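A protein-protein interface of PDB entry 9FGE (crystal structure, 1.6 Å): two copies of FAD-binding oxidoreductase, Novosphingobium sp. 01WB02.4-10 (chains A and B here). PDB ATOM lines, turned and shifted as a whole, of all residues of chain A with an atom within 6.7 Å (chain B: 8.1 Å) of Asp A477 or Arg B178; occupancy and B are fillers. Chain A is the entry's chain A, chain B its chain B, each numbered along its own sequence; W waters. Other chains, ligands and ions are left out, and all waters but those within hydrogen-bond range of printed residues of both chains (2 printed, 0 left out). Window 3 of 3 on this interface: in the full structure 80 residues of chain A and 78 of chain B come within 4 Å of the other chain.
Water W2 lies within hydrogen-bond range of ND2 of Asn A475 (2.7 Å) and N of Arg B181 (2.9 Å). Water W1 lies within hydrogen-bond range of OG1 of Thr A481, NH2 of Arg B178 and O of Asp A477.
OD2 of Asp A477 lies within salt-bridge range of NH1 of Arg B178 (3.0 Å). O of Arg B181 lies close to OD1 of Asn A475 (2.9 Å).
No position is printed for both chains. Of the 9 pairs that touch across the chains among the printed residues, none has its exchanged pair printed and touching as well.
O of Val B172 is in hydrogen-bond range of N of Met B180, at 2.8 Å. The side-chain carboxylate (OE2) of Glu B171 lies within salt-bridge range of the guanidinium group (NE) of Arg B181, 2.9 Å away. O of Asp A477 lies within hydrogen-bond range of OG1 of Thr A481, at 3.1 Å. OD2 of Asp B176 lies within salt-bridge range of NE of Arg B178 (2.9 Å).
Hydrophobic or aromatic side chains of chain B that line the printed part of chain A: Leu B174 and Met B180. Of the 11 printed residues of chain A, 4 touch a printed residue of chain B. Printed residues of chain A that touch a printed residue of chain B: Val A474, Asn A475, Asp A477 and Phe A478. Among the printed residues, 9 pairs touch across the chains.
Asp A477 touches just one residue of chain B: Arg B178. Arg B178 touches just these residues of chain A: Val A474 and Asp A477. Of the printed residues of chain A, Leu B174 touches Val A474 and Phe A478. Printed residues of chain A within 4 Å of Leu B179: Val A474. Printed residues of chain B within 4 Å of Phe A478: Leu B174 and Met B180. Of the printed residues of chain B, Asn A475 touches Met B180 and Arg B181. Printed residues of chain B within 4 Å of Val A474: Leu B174, Arg B178, Leu B179 and Met B180. The nearest residue of chain B that does not touch Asp A477 is Met B180 (6.9 Å). The nearest residue of chain A that does not touch Arg B178 is Phe A478 (5.0 Å). The nearest printed residue of chain B that does not touch Phe A478 is Arg B178 (5.0 Å).
Among the printed residues, merely in contact across the chains: Val A474 with Leu B174 (3.8 Å), Val A474 with Arg B178 (3.9 Å), Val A474 with Leu B179 (3.8 Å), Val A474 with Met B180 (3.8 Å), Asn A475 with Met B180 (3.7 Å), Phe A478 with Leu B174 (3.8 Å) and Phe A478 with Met B180 (3.7 Å).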
ATOM      1  N   GLY A 472      -5.899   4.365  20.253  1.00  0.00           N
ATOM      2  CA  GLY A 472      -6.143   2.996  19.798  1.00  0.00           C
ATOM      3  C   GLY A 472      -5.596   2.721  18.399  1.00  0.00           C
ATOM      4  O   GLY A 472      -5.583   3.580  17.511  1.00  0.00           O
ATOM      5  N   GLU A 473      -5.211   1.469  18.178  1.00  0.00           N
ATOM      6  CA  GLU A 473      -4.814   1.029  16.842  1.00  0.00           C
ATOM      7  C   GLU A 473      -5.976   1.097  15.855  1.00  0.00           C
ATOM      8  O   GLU A 473      -5.749   1.441  14.692  1.00  0.00           O
ATOM      9  CB  GLU A 473      -4.300  -0.413  16.859  1.00  0.00           C
ATOM     10  CG  GLU A 473      -3.006  -0.566  17.621  1.00  0.00           C
ATOM     11  CD  GLU A 473      -2.282  -1.874  17.348  1.00  0.00           C
ATOM     12  OE1 GLU A 473      -2.903  -2.780  16.735  1.00  0.00           O
ATOM     13  OE2 GLU A 473      -1.089  -1.959  17.705  1.00  0.00           O
ATOM     14  N   VAL A 474      -7.215   0.775  16.282  1.00  0.00           N
ATOM     15  CA  VAL A 474      -8.346   0.877  15.381  1.00  0.00           C
ATOM     16  C   VAL A 474      -8.545   2.335  14.956  1.00  0.00           C
ATOM     17  O   VAL A 474      -8.833   2.566  13.798  1.00  0.00           O
ATOM     18  CB  VAL A 474      -9.649   0.320  15.992  1.00  0.00           C
ATOM     19  CG1 VAL A 474     -10.852   0.467  15.089  1.00  0.00           C
ATOM     20  CG2 VAL A 474      -9.505  -1.173  16.298  1.00  0.00           C
ATOM     21  N   ASN A 475      -8.345   3.285  15.889  1.00  0.00           N
ATOM     22  CA  ASN A 475      -8.493   4.693  15.567  1.00  0.00           C
ATOM     23  C   ASN A 475      -7.490   5.089  14.489  1.00  0.00           C
ATOM     24  O   ASN A 475      -7.794   5.811  13.524  1.00  0.00           O
ATOM     25  CB  ASN A 475      -8.341   5.565  16.806  1.00  0.00           C
ATOM     26  CG  ASN A 475      -9.352   5.282  17.888  1.00  0.00           C
ATOM     27  OD1 ASN A 475     -10.260   6.114  18.180  1.00  0.00           O
ATOM     28  ND2 ASN A 475      -9.229   4.109  18.450  1.00  0.00           N
ATOM     29  N   ARG A 476      -6.242   4.625  14.684  1.00  0.00           N
ATOM     30  CA  ARG A 476      -5.174   4.929  13.729  1.00  0.00           C
ATOM     31  C   ARG A 476      -5.561   4.391  12.351  1.00  0.00           C
ATOM     32  O   ARG A 476      -5.444   5.082  11.325  1.00  0.00           O
ATOM     33  CB  ARG A 476      -3.858   4.328  14.246  1.00  0.00           C
ATOM     34  CG  ARG A 476      -2.562   4.849  13.664  1.00  0.00           C
ATOM     35  CD  ARG A 476      -2.080   6.057  14.454  1.00  0.00           C
ATOM     36  NE  ARG A 476      -0.970   6.709  13.741  1.00  0.00           N
ATOM     37  CZ  ARG A 476       0.325   6.508  13.979  1.00  0.00           C
ATOM     38  NH1 ARG A 476       0.747   5.641  14.904  1.00  0.00           N
ATOM     39  NH2 ARG A 476       1.208   7.208  13.308  1.00  0.00           N
ATOM     40  N   ASP A 477      -6.048   3.150  12.306  1.00  0.00           N
ATOM     41  CA  ASP A 477      -6.438   2.565  11.024  1.00  0.00           C
ATOM     42  C   ASP A 477      -7.604   3.292  10.363  1.00  0.00           C
ATOM     43  O   ASP A 477      -7.644   3.516   9.150  1.00  0.00           O
ATOM     44  CB  ASP A 477      -6.865   1.097  11.193  1.00  0.00           C
ATOM     45  CG  ASP A 477      -5.738   0.130  11.499  1.00  0.00           C
ATOM     46  OD1 ASP A 477      -4.577   0.527  11.340  1.00  0.00           O
ATOM     47  OD2 ASP A 477      -6.050  -1.024  11.958  1.00  0.00           O
ATOM     48  N   PHE A 478      -8.625   3.647  11.166  1.00  0.00           N
ATOM     49  CA  PHE A 478      -9.776   4.339  10.647  1.00  0.00           C
ATOM     50  C   PHE A 478      -9.380   5.718  10.076  1.00  0.00           C
ATOM     51  O   PHE A 478      -9.814   6.090   8.996  1.00  0.00           O
ATOM     52  CB  PHE A 478     -10.806   4.512  11.782  1.00  0.00           C
ATOM     53  CG  PHE A 478     -12.127   5.058  11.335  1.00  0.00           C
ATOM     54  CD1 PHE A 478     -13.044   4.230  10.715  1.00  0.00           C
ATOM     55  CD2 PHE A 478     -12.455   6.384  11.481  1.00  0.00           C
ATOM     56  CE1 PHE A 478     -14.287   4.725  10.347  1.00  0.00           C
ATOM     57  CE2 PHE A 478     -13.691   6.879  11.095  1.00  0.00           C
ATOM     58  CZ  PHE A 478     -14.599   6.027  10.517  1.00  0.00           C
ATOM     59  N   ASN A 479      -8.507   6.458  10.769  1.00  0.00           N
ATOM     60  CA  ASN A 479      -8.037   7.738  10.253  1.00  0.00           C
ATOM     61  C   ASN A 479      -7.326   7.526   8.910  1.00  0.00           C
ATOM     62  O   ASN A 479      -7.423   8.380   8.014  1.00  0.00           O
ATOM     63  CB  ASN A 479      -7.164   8.444  11.285  1.00  0.00           C
ATOM     64  CG  ASN A 479      -7.962   9.127  12.365  1.00  0.00           C
ATOM     65  OD1 ASN A 479      -9.091   9.521  12.156  1.00  0.00           O
ATOM     66  ND2 ASN A 479      -7.350   9.354  13.504  1.00  0.00           N
ATOM     67  N   ARG A 480      -6.571   6.435   8.783  1.00  0.00           N
ATOM     68  CA  ARG A 480      -5.838   6.185   7.554  1.00  0.00           C
ATOM     69  C   ARG A 480      -6.808   5.807   6.446  1.00  0.00           C
ATOM     70  O   ARG A 480      -6.599   6.187   5.302  1.00  0.00           O
ATOM     71  CB  ARG A 480      -4.734   5.143   7.771  1.00  0.00           C
ATOM     72  CG  ARG A 480      -3.739   5.020   6.631  1.00  0.00           C
ATOM     73  CD  ARG A 480      -2.566   4.162   7.074  1.00  0.00           C
ATOM     74  NE  ARG A 480      -1.338   4.636   6.426  1.00  0.00           N
ATOM     75  CZ  ARG A 480      -0.178   3.972   6.415  1.00  0.00           C
ATOM     76  NH1 ARG A 480      -0.108   2.745   6.915  1.00  0.00           N
ATOM     77  NH2 ARG A 480       0.898   4.523   5.878  1.00  0.00           N
ATOM     78  N   THR A 481      -7.872   5.062   6.757  1.00  0.00           N
ATOM     79  CA  THR A 481      -8.870   4.752   5.744  1.00  0.00           C
ATOM     80  C   THR A 481      -9.478   6.048   5.221  1.00  0.00           C
ATOM     81  O   THR A 481      -9.621   6.199   4.006  1.00  0.00           O
ATOM     82  CB  THR A 481      -9.990   3.848   6.285  1.00  0.00           C
ATOM     83  OG1 THR A 481      -9.337   2.632   6.654  1.00  0.00           O
ATOM     84  CG2 THR A 481     -11.117   3.622   5.295  1.00  0.00           C
ATOM     85  N   LEU A 482      -9.852   6.967   6.120  1.00  0.00           N
ATOM     86  CA  LEU A 482     -10.429   8.245   5.731  1.00  0.00           C
ATOM     87  C   LEU A 482      -9.426   9.024   4.873  1.00  0.00           C
ATOM     88  O   LEU A 482      -9.827   9.609   3.855  1.00  0.00           O
ATOM     89  CB  LEU A 482     -10.803   9.100   6.938  1.00  0.00           C
ATOM     90  CG  LEU A 482     -11.932   8.608   7.858  1.00  0.00           C
ATOM     91  CD1 LEU A 482     -12.090   9.526   9.077  1.00  0.00           C
ATOM     92  CD2 LEU A 482     -13.248   8.425   7.098  1.00  0.00           C
ATOM     93  N   VAL B  52     -22.853  -6.476  23.017  1.00  0.00           N
ATOM     94  CA  VAL B  52     -22.015  -5.895  21.983  1.00  0.00           C
ATOM     95  C   VAL B  52     -21.333  -7.016  21.194  1.00  0.00           C
ATOM     96  O   VAL B  52     -21.172  -6.898  19.986  1.00  0.00           O
ATOM     97  CB  VAL B  52     -21.032  -4.876  22.603  1.00  0.00           C
ATOM     98  CG1 VAL B  52     -20.024  -5.566  23.510  1.00  0.00           C
ATOM     99  CG2 VAL B  52     -20.326  -4.093  21.507  1.00  0.00           C
ATOM    100  N   GLN B  56     -21.377  -7.608  17.193  1.00  0.00           N
ATOM    101  CA  GLN B  56     -20.215  -7.721  16.300  1.00  0.00           C
ATOM    102  C   GLN B  56     -20.343  -8.951  15.375  1.00  0.00           C
ATOM    103  O   GLN B  56     -19.998  -8.936  14.175  1.00  0.00           O
ATOM    104  CB  GLN B  56     -18.903  -7.841  17.094  1.00  0.00           C
ATOM    105  CG  GLN B  56     -18.440  -6.570  17.811  1.00  0.00           C
ATOM    106  CD  GLN B  56     -17.229  -6.884  18.659  1.00  0.00           C
ATOM    107  OE1 GLN B  56     -17.327  -7.322  19.807  1.00  0.00           O
ATOM    108  NE2 GLN B  56     -16.060  -6.665  18.131  1.00  0.00           N
ATOM    109  N   VAL B  59     -22.782  -8.238  12.617  1.00  0.00           N
ATOM    110  CA  VAL B  59     -22.153  -7.440  11.568  1.00  0.00           C
ATOM    111  C   VAL B  59     -21.261  -8.289  10.679  1.00  0.00           C
ATOM    112  O   VAL B  59     -21.293  -8.117   9.429  1.00  0.00           O
ATOM    113  CB  VAL B  59     -21.430  -6.193  12.123  1.00  0.00           C
ATOM    114  CG1 VAL B  59     -20.646  -5.487  11.032  1.00  0.00           C
ATOM    115  CG2 VAL B  59     -22.452  -5.246  12.707  1.00  0.00           C
ATOM    116  N   ARG B  60     -20.487  -9.207  11.230  1.00  0.00           N
ATOM    117  CA  ARG B  60     -19.653 -10.086  10.398  1.00  0.00           C
ATOM    118  C   ARG B  60     -20.537 -10.888   9.446  1.00  0.00           C
ATOM    119  O   ARG B  60     -20.237 -10.987   8.244  1.00  0.00           O
ATOM    120  CB  ARG B  60     -18.796 -11.034  11.240  1.00  0.00           C
ATOM    121  CG  ARG B  60     -17.726 -10.281  12.026  1.00  0.00           C
ATOM    122  CD  ARG B  60     -17.008 -11.252  12.945  1.00  0.00           C
ATOM    123  NE  ARG B  60     -16.307 -10.465  13.940  1.00  0.00           N
ATOM    124  CZ  ARG B  60     -16.469 -10.551  15.252  1.00  0.00           C
ATOM    125  NH1 ARG B  60     -17.332 -11.399  15.778  1.00  0.00           N
ATOM    126  NH2 ARG B  60     -15.753  -9.751  16.024  1.00  0.00           N
ATOM    127  N   ASN B  63     -21.953  -8.865   6.480  1.00  0.00           N
ATOM    128  CA  ASN B  63     -20.968  -8.733   5.416  1.00  0.00           C
ATOM    129  C   ASN B  63     -20.903  -9.989   4.532  1.00  0.00           C
ATOM    130  O   ASN B  63     -20.950  -9.925   3.300  1.00  0.00           O
ATOM    131  CB  ASN B  63     -19.613  -8.355   6.008  1.00  0.00           C
ATOM    132  CG  ASN B  63     -19.561  -6.875   6.348  1.00  0.00           C
ATOM    133  OD1 ASN B  63     -19.389  -6.001   5.495  1.00  0.00           O
ATOM    134  ND2 ASN B  63     -19.656  -6.543   7.630  1.00  0.00           N
ATOM    135  N   GLU B 171     -18.668   4.485  21.847  1.00  0.00           N
ATOM    136  CA  GLU B 171     -18.116   3.290  21.228  1.00  0.00           C
ATOM    137  C   GLU B 171     -18.970   2.927  20.022  1.00  0.00           C
ATOM    138  O   GLU B 171     -20.206   2.986  20.068  1.00  0.00           O
ATOM    139  CB  GLU B 171     -18.140   2.105  22.191  1.00  0.00           C
ATOM    140  CG  GLU B 171     -17.533   0.802  21.666  1.00  0.00           C
ATOM    141  CD  GLU B 171     -17.640  -0.317  22.699  1.00  0.00           C
ATOM    142  OE1 GLU B 171     -18.762  -0.877  22.899  1.00  0.00           O
ATOM    143  OE2 GLU B 171     -16.622  -0.522  23.409  1.00  0.00           O
ATOM    144  N   VAL B 172     -18.288   2.578  18.928  1.00  0.00           N
ATOM    145  CA  VAL B 172     -18.939   2.255  17.666  1.00  0.00           C
ATOM    146  C   VAL B 172     -18.439   0.901  17.202  1.00  0.00           C
ATOM    147  O   VAL B 172     -17.235   0.607  17.257  1.00  0.00           O
ATOM    148  CB  VAL B 172     -18.570   3.313  16.609  1.00  0.00           C
ATOM    149  CG1 VAL B 172     -19.217   3.019  15.294  1.00  0.00           C
ATOM    150  CG2 VAL B 172     -18.935   4.726  17.079  1.00  0.00           C
ATOM    151  N   CYS B 173     -19.364   0.049  16.758  1.00  0.00           N
ATOM    152  CA  CYS B 173     -19.024  -1.105  15.938  1.00  0.00           C
ATOM    153  C   CYS B 173     -18.973  -0.623  14.492  1.00  0.00           C
ATOM    154  O   CYS B 173     -19.997  -0.190  13.939  1.00  0.00           O
ATOM    155  CB  CYS B 173     -20.059  -2.221  16.154  1.00  0.00           C
ATOM    156  SG  CYS B 173     -19.696  -3.753  15.218  1.00  0.00           S
ATOM    157  N   LEU B 174     -17.770  -0.664  13.900  1.00  0.00           N
ATOM    158  CA  LEU B 174     -17.565  -0.302  12.493  1.00  0.00           C
ATOM    159  C   LEU B 174     -18.159  -1.374  11.587  1.00  0.00           C
ATOM    160  O   LEU B 174     -18.493  -2.480  12.051  1.00  0.00           O
ATOM    161  CB  LEU B 174     -16.080  -0.122  12.259  1.00  0.00           C
ATOM    162  CG  LEU B 174     -15.483   0.993  13.113  1.00  0.00           C
ATOM    163  CD1 LEU B 174     -13.976   0.960  12.984  1.00  0.00           C
ATOM    164  CD2 LEU B 174     -16.069   2.350  12.738  1.00  0.00           C
ATOM    165  N   PRO B 175     -18.358  -1.051  10.305  1.00  0.00           N
ATOM    166  CA  PRO B 175     -18.929  -2.026   9.376  1.00  0.00           C
ATOM    167  C   PRO B 175     -18.189  -3.334   9.252  1.00  0.00           C
ATOM    168  O   PRO B 175     -18.815  -4.256   8.822  1.00  0.00           O
ATOM    169  CB  PRO B 175     -18.882  -1.243   8.066  1.00  0.00           C
ATOM    170  CG  PRO B 175     -19.168   0.149   8.505  1.00  0.00           C
ATOM    171  CD  PRO B 175     -18.248   0.282   9.683  1.00  0.00           C
ATOM    172  N   ASP B 176     -16.907  -3.393   9.631  1.00  0.00           N
ATOM    173  CA  ASP B 176     -16.143  -4.644   9.568  1.00  0.00           C
ATOM    174  C   ASP B 176     -16.270  -5.468  10.859  1.00  0.00           C
ATOM    175  O   ASP B 176     -15.612  -6.499  10.994  1.00  0.00           O
ATOM    176  CB  ASP B 176     -14.670  -4.383   9.285  1.00  0.00           C
ATOM    177  CG  ASP B 176     -13.888  -3.611  10.343  1.00  0.00           C
ATOM    178  OD1 ASP B 176     -14.471  -3.143  11.317  1.00  0.00           O
ATOM    179  OD2 ASP B 176     -12.681  -3.431  10.170  1.00  0.00           O
ATOM    180  N   GLY B 177     -16.972  -4.963  11.876  1.00  0.00           N
ATOM    181  CA  GLY B 177     -17.145  -5.696  13.111  1.00  0.00           C
ATOM    182  C   GLY B 177     -16.167  -5.334  14.226  1.00  0.00           C
ATOM    183  O   GLY B 177     -16.287  -5.875  15.321  1.00  0.00           O
ATOM    184  N   ARG B 178     -15.190  -4.440  13.966  1.00  0.00           N
ATOM    185  CA  ARG B 178     -14.299  -3.960  15.020  1.00  0.00           C
ATOM    186  C   ARG B 178     -14.948  -2.854  15.851  1.00  0.00           C
ATOM    187  O   ARG B 178     -15.691  -2.056  15.310  1.00  0.00           O
ATOM    188  CB  ARG B 178     -13.018  -3.445  14.357  1.00  0.00           C
ATOM    189  CG  ARG B 178     -12.201  -4.572  13.728  1.00  0.00           C
ATOM    190  CD  ARG B 178     -10.803  -4.094  13.341  1.00  0.00           C
ATOM    191  NE  ARG B 178     -10.880  -2.994  12.389  1.00  0.00           N
ATOM    192  CZ  ARG B 178      -9.863  -2.184  12.070  1.00  0.00           C
ATOM    193  NH1 ARG B 178      -8.689  -2.330  12.648  1.00  0.00           N
ATOM    194  NH2 ARG B 178     -10.067  -1.171  11.247  1.00  0.00           N
ATOM    195  N   LEU B 179     -14.597  -2.767  17.122  1.00  0.00           N
ATOM    196  CA  LEU B 179     -15.086  -1.698  17.984  1.00  0.00           C
ATOM    197  C   LEU B 179     -14.052  -0.574  17.971  1.00  0.00           C
ATOM    198  O   LEU B 179     -12.843  -0.818  18.027  1.00  0.00           O
ATOM    199  CB  LEU B 179     -15.303  -2.203  19.408  1.00  0.00           C
ATOM    200  CG  LEU B 179     -16.324  -3.334  19.569  1.00  0.00           C
ATOM    201  CD1 LEU B 179     -16.450  -3.743  21.009  1.00  0.00           C
ATOM    202  CD2 LEU B 179     -17.670  -2.926  19.023  1.00  0.00           C
ATOM    203  N   MET B 180     -14.549   0.633  17.913  1.00  0.00           N
ATOM    204  CA  MET B 180     -13.725   1.841  18.100  1.00  0.00           C
ATOM    205  C   MET B 180     -14.327   2.771  19.158  1.00  0.00           C
ATOM    206  O   MET B 180     -15.521   3.112  19.118  1.00  0.00           O
ATOM    207  CB  MET B 180     -13.615   2.549  16.752  1.00  0.00           C
ATOM    208  CG  MET B 180     -12.683   3.744  16.735  1.00  0.00           C
ATOM    209  SD  MET B 180     -12.513   4.511  15.117  1.00  0.00           S
ATOM    210  CE  MET B 180     -14.057   5.414  15.021  1.00  0.00           C
ATOM    211  N   ARG B 181     -13.473   3.270  20.098  1.00  0.00           N
ATOM    212  CA  ARG B 181     -13.905   4.274  21.073  1.00  0.00           C
ATOM    213  C   ARG B 181     -13.366   5.650  20.717  1.00  0.00           C
ATOM    214  O   ARG B 181     -12.182   5.801  20.394  1.00  0.00           O
ATOM    215  CB  ARG B 181     -13.484   3.855  22.479  1.00  0.00           C
ATOM    216  CG  ARG B 181     -14.149   2.548  22.950  1.00  0.00           C
ATOM    217  CD  ARG B 181     -13.884   2.294  24.418  1.00  0.00           C
ATOM    218  NE  ARG B 181     -14.720   1.165  24.830  1.00  0.00           N
ATOM    219  CZ  ARG B 181     -14.873   0.745  26.071  1.00  0.00           C
ATOM    220  NH1 ARG B 181     -14.260   1.356  27.067  1.00  0.00           N
ATOM    221  NH2 ARG B 181     -15.736  -0.241  26.305  1.00  0.00           N
ATOM    222  N   GLY B 214     -21.630   3.651  11.155  1.00  0.00           N
ATOM    223  CA  GLY B 214     -21.315   2.762  12.261  1.00  0.00           C
ATOM    224  C   GLY B 214     -22.535   2.488  13.111  1.00  0.00           C
ATOM    225  O   GLY B 214     -23.517   3.189  12.985  1.00  0.00           O
ATOM    226  N   ILE B 215     -22.428   1.489  13.987  1.00  0.00           N
ATOM    227  CA  ILE B 215     -23.434   1.154  14.986  1.00  0.00           C
ATOM    228  C   ILE B 215     -22.917   1.604  16.347  1.00  0.00           C
ATOM    229  O   ILE B 215     -21.900   1.090  16.822  1.00  0.00           O
ATOM    230  CB  ILE B 215     -23.671  -0.368  14.973  1.00  0.00           C
ATOM    231  CG1 ILE B 215     -24.215  -0.794  13.615  1.00  0.00           C
ATOM    232  CG2 ILE B 215     -24.620  -0.769  16.099  1.00  0.00           C
ATOM    233  CD1 ILE B 215     -24.087  -2.303  13.406  1.00  0.00           C
ATOM    234  N   THR B 217     -22.661   1.530  20.140  1.00  0.00           N
ATOM    235  CA  THR B 217     -22.916   0.525  21.153  1.00  0.00           C
ATOM    236  C   THR B 217     -22.841   1.060  22.571  1.00  0.00           C
ATOM    237  O   THR B 217     -23.403   0.414  23.477  1.00  0.00           O
ATOM    238  CB  THR B 217     -21.920  -0.620  21.000  1.00  0.00           C
ATOM    239  OG1 THR B 217     -20.571  -0.120  21.022  1.00  0.00           O
ATOM    240  CG2 THR B 217     -22.192  -1.350  19.709  1.00  0.00           C
HETATM  241  O   HOH W   1      -9.926   1.082   8.941  1.00  0.00           O
HETATM  242  O   HOH W   2     -10.766   2.371  19.895  1.00  0.00           O
